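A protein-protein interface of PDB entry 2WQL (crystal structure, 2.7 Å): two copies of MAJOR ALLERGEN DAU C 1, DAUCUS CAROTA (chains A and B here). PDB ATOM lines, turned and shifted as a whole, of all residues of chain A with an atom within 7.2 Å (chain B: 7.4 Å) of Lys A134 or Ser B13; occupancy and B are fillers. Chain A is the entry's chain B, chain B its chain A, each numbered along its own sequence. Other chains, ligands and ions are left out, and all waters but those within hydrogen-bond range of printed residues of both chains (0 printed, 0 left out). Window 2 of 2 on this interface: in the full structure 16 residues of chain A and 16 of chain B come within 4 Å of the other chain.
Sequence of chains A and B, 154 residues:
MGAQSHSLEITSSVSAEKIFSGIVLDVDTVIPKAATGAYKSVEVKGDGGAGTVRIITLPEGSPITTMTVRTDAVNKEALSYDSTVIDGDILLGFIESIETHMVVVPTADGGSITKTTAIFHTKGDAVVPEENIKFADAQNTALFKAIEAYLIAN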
ATOM      1  N   HIS A   6     -22.637   0.612  -1.309  1.00  0.00           N
ATOM      2  CA  HIS A   6     -22.310   1.863  -1.977  1.00  0.00           C
ATOM      3  C   HIS A   6     -23.561   2.434  -2.620  1.00  0.00           C
ATOM      4  O   HIS A   6     -24.398   1.688  -3.083  1.00  0.00           O
ATOM      5  CB  HIS A   6     -21.238   1.633  -3.054  1.00  0.00           C
ATOM      6  CG  HIS A   6     -20.899   2.858  -3.828  1.00  0.00           C
ATOM      7  ND1 HIS A   6     -20.155   3.888  -3.297  1.00  0.00           N
ATOM      8  CD2 HIS A   6     -21.226   3.235  -5.090  1.00  0.00           C
ATOM      9  CE1 HIS A   6     -20.028   4.847  -4.202  1.00  0.00           C
ATOM     10  NE2 HIS A   6     -20.669   4.476  -5.299  1.00  0.00           N
ATOM     11  N   PRO A 129     -12.408  -3.161  -3.962  1.00  0.00           N
ATOM     12  CA  PRO A 129     -11.645  -1.917  -3.952  1.00  0.00           C
ATOM     13  C   PRO A 129     -12.397  -0.716  -4.504  1.00  0.00           C
ATOM     14  O   PRO A 129     -13.229  -0.852  -5.386  1.00  0.00           O
ATOM     15  CB  PRO A 129     -10.440  -2.233  -4.844  1.00  0.00           C
ATOM     16  CG  PRO A 129     -10.340  -3.688  -4.858  1.00  0.00           C
ATOM     17  CD  PRO A 129     -11.733  -4.190  -4.775  1.00  0.00           C
ATOM     18  N   GLU A 130     -12.064   0.457  -3.988  1.00  0.00           N
ATOM     19  CA  GLU A 130     -12.694   1.707  -4.397  1.00  0.00           C
ATOM     20  C   GLU A 130     -12.574   1.980  -5.926  1.00  0.00           C
ATOM     21  O   GLU A 130     -13.526   2.471  -6.544  1.00  0.00           O
ATOM     22  CB  GLU A 130     -12.134   2.867  -3.545  1.00  0.00           C
ATOM     23  CG  GLU A 130     -12.974   4.177  -3.518  1.00  0.00           C
ATOM     24  CD  GLU A 130     -14.441   3.996  -3.021  1.00  0.00           C
ATOM     25  OE1 GLU A 130     -14.698   3.052  -2.216  1.00  0.00           O
ATOM     26  OE2 GLU A 130     -15.337   4.799  -3.448  1.00  0.00           O
ATOM     27  N   GLU A 131     -11.449   1.618  -6.542  1.00  0.00           N
ATOM     28  CA  GLU A 131     -11.274   1.843  -7.986  1.00  0.00           C
ATOM     29  C   GLU A 131     -12.344   1.099  -8.801  1.00  0.00           C
ATOM     30  O   GLU A 131     -12.856   1.642  -9.772  1.00  0.00           O
ATOM     31  CB  GLU A 131      -9.829   1.535  -8.478  1.00  0.00           C
ATOM     32  CG  GLU A 131      -9.485   0.036  -8.779  1.00  0.00           C
ATOM     33  CD  GLU A 131      -8.268  -0.165  -9.729  1.00  0.00           C
ATOM     34  OE1 GLU A 131      -8.343   0.254 -10.919  1.00  0.00           O
ATOM     35  OE2 GLU A 131      -7.262  -0.785  -9.286  1.00  0.00           O
ATOM     36  N   ASN A 132     -12.708  -0.113  -8.396  1.00  0.00           N
ATOM     37  CA  ASN A 132     -13.708  -0.891  -9.144  1.00  0.00           C
ATOM     38  C   ASN A 132     -15.100  -0.313  -9.013  1.00  0.00           C
ATOM     39  O   ASN A 132     -15.897  -0.376  -9.950  1.00  0.00           O
ATOM     40  CB  ASN A 132     -13.722  -2.348  -8.707  1.00  0.00           C
ATOM     41  CG  ASN A 132     -12.410  -3.019  -8.931  1.00  0.00           C
ATOM     42  OD1 ASN A 132     -11.490  -2.899  -8.126  1.00  0.00           O
ATOM     43  ND2 ASN A 132     -12.306  -3.728 -10.035  1.00  0.00           N
ATOM     44  N   ILE A 133     -15.392   0.250  -7.847  1.00  0.00           N
ATOM     45  CA  ILE A 133     -16.684   0.880  -7.600  1.00  0.00           C
ATOM     46  C   ILE A 133     -16.810   2.202  -8.382  1.00  0.00           C
ATOM     47  O   ILE A 133     -17.853   2.493  -8.966  1.00  0.00           O
ATOM     48  CB  ILE A 133     -16.903   1.132  -6.094  1.00  0.00           C
ATOM     49  CG1 ILE A 133     -16.953  -0.202  -5.335  1.00  0.00           C
ATOM     50  CG2 ILE A 133     -18.184   1.941  -5.859  1.00  0.00           C
ATOM     51  CD1 ILE A 133     -16.811  -0.038  -3.821  1.00  0.00           C
ATOM     52  N   LYS A 134     -15.742   2.993  -8.401  1.00  0.00           N
ATOM     53  CA  LYS A 134     -15.726   4.205  -9.208  1.00  0.00           C
ATOM     54  C   LYS A 134     -15.897   3.902 -10.690  1.00  0.00           C
ATOM     55  O   LYS A 134     -16.608   4.629 -11.388  1.00  0.00           O
ATOM     56  CB  LYS A 134     -14.436   4.975  -9.016  1.00  0.00           C
ATOM     57  CG  LYS A 134     -14.321   5.737  -7.699  1.00  0.00           C
ATOM     58  CD  LYS A 134     -12.877   6.284  -7.557  1.00  0.00           C
ATOM     59  CE  LYS A 134     -12.645   7.103  -6.273  1.00  0.00           C
ATOM     60  NZ  LYS A 134     -11.266   7.705  -6.225  1.00  0.00           N
ATOM     61  N   PHE A 135     -15.255   2.835 -11.166  1.00  0.00           N
ATOM     62  CA  PHE A 135     -15.387   2.418 -12.556  1.00  0.00           C
ATOM     63  C   PHE A 135     -16.839   2.146 -12.898  1.00  0.00           C
ATOM     64  O   PHE A 135     -17.353   2.653 -13.897  1.00  0.00           O
ATOM     65  CB  PHE A 135     -14.557   1.161 -12.844  1.00  0.00           C
ATOM     66  CG  PHE A 135     -14.673   0.681 -14.264  1.00  0.00           C
ATOM     67  CD1 PHE A 135     -13.913   1.261 -15.266  1.00  0.00           C
ATOM     68  CD2 PHE A 135     -15.566  -0.320 -14.603  1.00  0.00           C
ATOM     69  CE1 PHE A 135     -14.029   0.846 -16.576  1.00  0.00           C
ATOM     70  CE2 PHE A 135     -15.692  -0.740 -15.918  1.00  0.00           C
ATOM     71  CZ  PHE A 135     -14.921  -0.158 -16.904  1.00  0.00           C
ATOM     72  N   ALA A 136     -17.491   1.329 -12.074  1.00  0.00           N
ATOM     73  CA  ALA A 136     -18.906   0.998 -12.267  1.00  0.00           C
ATOM     74  C   ALA A 136     -19.762   2.273 -12.315  1.00  0.00           C
ATOM     75  O   ALA A 136     -20.612   2.420 -13.180  1.00  0.00           O
ATOM     76  CB  ALA A 136     -19.397   0.058 -11.176  1.00  0.00           C
ATOM     77  N   ASP A 137     -19.522   3.197 -11.392  1.00  0.00           N
ATOM     78  CA  ASP A 137     -20.280   4.444 -11.343  1.00  0.00           C
ATOM     79  C   ASP A 137     -20.132   5.263 -12.626  1.00  0.00           C
ATOM     80  O   ASP A 137     -21.115   5.816 -13.133  1.00  0.00           O
ATOM     81  CB  ASP A 137     -19.831   5.294 -10.156  1.00  0.00           C
ATOM     82  CG  ASP A 137     -20.323   4.746  -8.807  1.00  0.00           C
ATOM     83  OD1 ASP A 137     -21.143   3.787  -8.783  1.00  0.00           O
ATOM     84  OD2 ASP A 137     -19.870   5.279  -7.754  1.00  0.00           O
ATOM     85  N   ALA A 138     -18.907   5.348 -13.134  1.00  0.00           N
ATOM     86  CA  ALA A 138     -18.648   6.085 -14.355  1.00  0.00           C
ATOM     87  C   ALA A 138     -19.409   5.448 -15.508  1.00  0.00           C
ATOM     88  O   ALA A 138     -20.069   6.136 -16.279  1.00  0.00           O
ATOM     89  CB  ALA A 138     -17.168   6.130 -14.655  1.00  0.00           C
ATOM     90  N   GLN A 139     -19.340   4.132 -15.607  1.00  0.00           N
ATOM     91  CA  GLN A 139     -19.889   3.441 -16.747  1.00  0.00           C
ATOM     92  C   GLN A 139     -21.422   3.423 -16.725  1.00  0.00           C
ATOM     93  O   GLN A 139     -22.060   3.574 -17.759  1.00  0.00           O
ATOM     94  CB  GLN A 139     -19.314   2.034 -16.792  1.00  0.00           C
ATOM     95  CG  GLN A 139     -19.706   1.219 -18.024  1.00  0.00           C
ATOM     96  CD  GLN A 139     -18.578   0.315 -18.480  1.00  0.00           C
ATOM     97  OE1 GLN A 139     -17.580   0.788 -19.065  1.00  0.00           O
ATOM     98  NE2 GLN A 139     -18.723  -0.994 -18.216  1.00  0.00           N
ATOM     99  N   ASN A 140     -22.000   3.268 -15.537  1.00  0.00           N
ATOM    100  CA  ASN A 140     -23.447   3.344 -15.352  1.00  0.00           C
ATOM    101  C   ASN A 140     -23.979   4.747 -15.619  1.00  0.00           C
ATOM    102  O   ASN A 140     -25.072   4.907 -16.152  1.00  0.00           O
ATOM    103  CB  ASN A 140     -23.836   2.919 -13.930  1.00  0.00           C
ATOM    104  CG  ASN A 140     -23.805   1.414 -13.732  1.00  0.00           C
ATOM    105  OD1 ASN A 140     -24.253   0.647 -14.597  1.00  0.00           O
ATOM    106  ND2 ASN A 140     -23.282   0.975 -12.575  1.00  0.00           N
ATOM    107  N   THR B  11     -18.577  17.143 -12.711  1.00  0.00           N
ATOM    108  CA  THR B  11     -17.716  16.785 -11.595  1.00  0.00           C
ATOM    109  C   THR B  11     -17.149  15.380 -11.783  1.00  0.00           C
ATOM    110  O   THR B  11     -17.826  14.491 -12.306  1.00  0.00           O
ATOM    111  CB  THR B  11     -18.505  16.855 -10.265  1.00  0.00           C
ATOM    112  OG1 THR B  11     -18.908  18.209 -10.043  1.00  0.00           O
ATOM    113  CG2 THR B  11     -17.666  16.424  -9.086  1.00  0.00           C
ATOM    114  N   SER B  12     -15.907  15.194 -11.349  1.00  0.00           N
ATOM    115  CA  SER B  12     -15.240  13.906 -11.414  1.00  0.00           C
ATOM    116  C   SER B  12     -14.324  13.710 -10.221  1.00  0.00           C
ATOM    117  O   SER B  12     -13.760  14.655  -9.711  1.00  0.00           O
ATOM    118  CB  SER B  12     -14.415  13.791 -12.698  1.00  0.00           C
ATOM    119  OG  SER B  12     -13.713  12.551 -12.760  1.00  0.00           O
ATOM    120  N   SER B  13     -14.165  12.468  -9.791  1.00  0.00           N
ATOM    121  CA  SER B  13     -13.217  12.138  -8.734  1.00  0.00           C
ATOM    122  C   SER B  13     -11.813  11.964  -9.285  1.00  0.00           C
ATOM    123  O   SER B  13     -10.872  11.879  -8.506  1.00  0.00           O
ATOM    124  CB  SER B  13     -13.634  10.861  -7.999  1.00  0.00           C
ATOM    125  OG  SER B  13     -13.672   9.753  -8.873  1.00  0.00           O
ATOM    126  N   VAL B  14     -11.677  11.885 -10.609  1.00  0.00           N
ATOM    127  CA  VAL B  14     -10.377  11.809 -11.260  1.00  0.00           C
ATOM    128  C   VAL B  14      -9.732  13.205 -11.287  1.00  0.00           C
ATOM    129  O   VAL B  14     -10.424  14.222 -11.366  1.00  0.00           O
ATOM    130  CB  VAL B  14     -10.493  11.260 -12.704  1.00  0.00           C
ATOM    131  CG1 VAL B  14      -9.162  11.346 -13.419  1.00  0.00           C
ATOM    132  CG2 VAL B  14     -11.009   9.830 -12.700  1.00  0.00           C
ATOM    133  N   SER B  15      -8.407  13.253 -11.229  1.00  0.00           N
ATOM    134  CA  SER B  15      -7.685  14.524 -11.154  1.00  0.00           C
ATOM    135  C   SER B  15      -7.800  15.326 -12.443  1.00  0.00           C
ATOM    136  O   SER B  15      -8.066  14.778 -13.506  1.00  0.00           O
ATOM    137  CB  SER B  15      -6.212  14.279 -10.830  1.00  0.00           C
ATOM    138  OG  SER B  15      -5.515  13.820 -11.971  1.00  0.00           O
ATOM    139  N   ALA B  16      -7.574  16.626 -12.317  1.00  0.00           N
ATOM    140  CA  ALA B  16      -7.660  17.579 -13.431  1.00  0.00           C
ATOM    141  C   ALA B  16      -6.692  17.265 -14.570  1.00  0.00           C
ATOM    142  O   ALA B  16      -7.082  17.294 -15.738  1.00  0.00           O
ATOM    143  CB  ALA B  16      -7.429  19.022 -12.910  1.00  0.00           C
ATOM    144  N   ILE B  19      -7.968  13.995 -16.373  1.00  0.00           N
ATOM    145  CA  ILE B  19      -9.182  14.229 -17.153  1.00  0.00           C
ATOM    146  C   ILE B  19      -8.854  14.965 -18.445  1.00  0.00           C
ATOM    147  O   ILE B  19      -9.281  14.568 -19.531  1.00  0.00           O
ATOM    148  CB  ILE B  19     -10.232  15.036 -16.350  1.00  0.00           C
ATOM    149  CG1 ILE B  19     -10.927  14.137 -15.327  1.00  0.00           C
ATOM    150  CG2 ILE B  19     -11.289  15.627 -17.254  1.00  0.00           C
ATOM    151  CD1 ILE B  19     -11.844  13.105 -15.938  1.00  0.00           C
ATOM    152  N   ASP B 109     -10.582  17.795  -2.887  1.00  0.00           N
ATOM    153  CA  ASP B 109     -10.559  16.341  -2.666  1.00  0.00           C
ATOM    154  C   ASP B 109      -9.630  15.568  -3.620  1.00  0.00           C
ATOM    155  O   ASP B 109      -9.548  14.340  -3.547  1.00  0.00           O
ATOM    156  CB  ASP B 109     -11.989  15.762  -2.718  1.00  0.00           C
ATOM    157  CG  ASP B 109     -12.700  16.018  -4.048  1.00  0.00           C
ATOM    158  OD1 ASP B 109     -12.040  16.447  -5.040  1.00  0.00           O
ATOM    159  OD2 ASP B 109     -13.939  15.791  -4.093  1.00  0.00           O
ATOM    160  N   GLY B 110      -8.940  16.271  -4.517  1.00  0.00           N
ATOM    161  CA  GLY B 110      -8.072  15.614  -5.499  1.00  0.00           C
ATOM    162  C   GLY B 110      -8.791  15.263  -6.790  1.00  0.00           C
ATOM    163  O   GLY B 110      -8.184  14.674  -7.686  1.00  0.00           O
ATOM    164  N   GLY B 111     -10.074  15.616  -6.887  1.00  0.00           N
ATOM    165  CA  GLY B 111     -10.834  15.454  -8.118  1.00  0.00           C
ATOM    166  C   GLY B 111     -10.824  16.725  -8.935  1.00  0.00           C
ATOM    167  O   GLY B 111      -9.898  17.529  -8.810  1.00  0.00           O
ATOM    168  N   SER B 112     -11.851  16.904  -9.768  1.00  0.00           N
ATOM    169  CA  SER B 112     -11.910  18.033 -10.690  1.00  0.00           C
ATOM    170  C   SER B 112     -13.328  18.425 -11.104  1.00  0.00           C
ATOM    171  O   SER B 112     -14.256  17.650 -10.951  1.00  0.00           O
ATOM    172  CB  SER B 112     -11.100  17.701 -11.945  1.00  0.00           C
ATOM    173  OG  SER B 112     -11.586  16.519 -12.590  1.00  0.00           O
ATOM    174  N   PHE B 144     -18.024  12.057 -21.768  1.00  0.00           N
ATOM    175  CA  PHE B 144     -17.115  12.387 -20.671  1.00  0.00           C
ATOM    176  C   PHE B 144     -16.960  11.208 -19.716  1.00  0.00           C
ATOM    177  O   PHE B 144     -15.839  10.814 -19.380  1.00  0.00           O
ATOM    178  CB  PHE B 144     -17.637  13.595 -19.888  1.00  0.00           C
ATOM    179  CG  PHE B 144     -16.745  14.023 -18.758  1.00  0.00           C
ATOM    180  CD1 PHE B 144     -15.863  15.086 -18.921  1.00  0.00           C
ATOM    181  CD2 PHE B 144     -16.774  13.382 -17.546  1.00  0.00           C
ATOM    182  CE1 PHE B 144     -15.039  15.496 -17.897  1.00  0.00           C
ATOM    183  CE2 PHE B 144     -15.945  13.778 -16.518  1.00  0.00           C
ATOM    184  CZ  PHE B 144     -15.075  14.848 -16.699  1.00  0.00           C
ATOM    185  N   LYS B 145     -18.091  10.650 -19.289  1.00  0.00           N
ATOM    186  CA  LYS B 145     -18.101   9.606 -18.287  1.00  0.00           C
ATOM    187  C   LYS B 145     -17.598   8.266 -18.812  1.00  0.00           C
ATOM    188  O   LYS B 145     -17.045   7.465 -18.062  1.00  0.00           O
ATOM    189  CB  LYS B 145     -19.501   9.467 -17.681  1.00  0.00           C
ATOM    190  CG  LYS B 145     -19.921  10.647 -16.780  1.00  0.00           C
ATOM    191  CD  LYS B 145     -19.007  10.779 -15.558  1.00  0.00           C
ATOM    192  CE  LYS B 145     -19.508  11.794 -14.524  1.00  0.00           C
ATOM    193  NZ  LYS B 145     -18.521  11.910 -13.380  1.00  0.00           N
ATOM    194  N   GLU B 148     -13.971   8.890 -18.452  1.00  0.00           N
ATOM    195  CA  GLU B 148     -13.643   8.757 -17.024  1.00  0.00           C
ATOM    196  C   GLU B 148     -13.477   7.279 -16.620  1.00  0.00           C
ATOM    197  O   GLU B 148     -12.545   6.905 -15.913  1.00  0.00           O
ATOM    198  CB  GLU B 148     -14.721   9.418 -16.163  1.00  0.00           C
ATOM    199  CG  GLU B 148     -14.269   9.760 -14.757  1.00  0.00           C
ATOM    200  CD  GLU B 148     -15.426  10.068 -13.811  1.00  0.00           C
ATOM    201  OE1 GLU B 148     -15.692   9.228 -12.937  1.00  0.00           O
ATOM    202  OE2 GLU B 148     -16.080  11.131 -13.930  1.00  0.00           O
ATOM    203  N   ALA B 149     -14.381   6.439 -17.093  1.00  0.00           N
ATOM    204  CA  ALA B 149     -14.322   5.011 -16.814  1.00  0.00           C
ATOM    205  C   ALA B 149     -13.029   4.398 -17.340  1.00  0.00           C
ATOM    206  O   ALA B 149     -12.378   3.608 -16.660  1.00  0.00           O
ATOM    207  CB  ALA B 149     -15.513   4.320 -17.415  1.00  0.00           C
ATOM    208  N   ILE B 152     -10.057   5.552 -15.105  1.00  0.00           N
ATOM    209  CA  ILE B 152     -10.014   4.901 -13.808  1.00  0.00           C
ATOM    210  C   ILE B 152      -9.414   3.486 -13.923  1.00  0.00           C
ATOM    211  O   ILE B 152      -8.764   3.008 -12.994  1.00  0.00           O
ATOM    212  CB  ILE B 152     -11.407   4.838 -13.168  1.00  0.00           C
ATOM    213  CG1 ILE B 152     -11.845   6.238 -12.741  1.00  0.00           C
ATOM    214  CG2 ILE B 152     -11.425   3.874 -11.973  1.00  0.00           C
ATOM    215  CD1 ILE B 152     -13.349   6.362 -12.495  1.00  0.00           C
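No position is printed for both chains.
OE1 of Glu A131 sits close to O of Ile B152.
Of the 13 printed residues of chain A, 4 touch a printed residue of chain B. Printed residues of chain A that touch a printed residue of chain B: Glu A131, Lys A134, Phe A135 and Ala A138. Of the 16 printed residues of chain B, 5 touch a printed residue of chain A. Printed residues of chain B that touch a printed residue of chain A: Ser B13, Lys B145, Glu B148, Ala B149 and Ile B152. Among the printed residues, 7 pairs touch across the chains. Among the printed residues, no Asp or Glu carboxylate lies within 4 Å of a Lys or Arg side-chain nitrogen of the other chain.
Lys A134 touches two residues of chain B. Ser B13 touches just one residue of chain A: Lys A134. Of the printed residues of chain B, Phe A135 touches Ala B149 (3.1 Å). Printed residues of chain A within 4 Å of Glu B148: Ala A138. Printed residues of chain B within 4 Å of Glu A131: Ile B152. The nearest residue of chain B that does not touch Lys A134 is Glu B148 (4.9 Å).
The side-chain amino group (NZ) of Lys B145 sits at hydrogen-bond distance from the backbone carbonyl oxygen (O) of Thr B11. OE2 of Glu B148 sits at hydrogen-bond distance from OG of Ser B12 (3.0 Å). The side-chain carboxylate of Glu B148 is in salt-bridge range of the side-chain amino group of Lys B145, 2.6 Å away.
Among the printed residues, merely in contact across the chains: Lys A134 with Ser B13, Lys A134 with Ile B152, Phe A135 with Ala B149, Ala A138 with Lys B145, Ala A138 with Glu B148 and Ala A138 with Ala B149.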
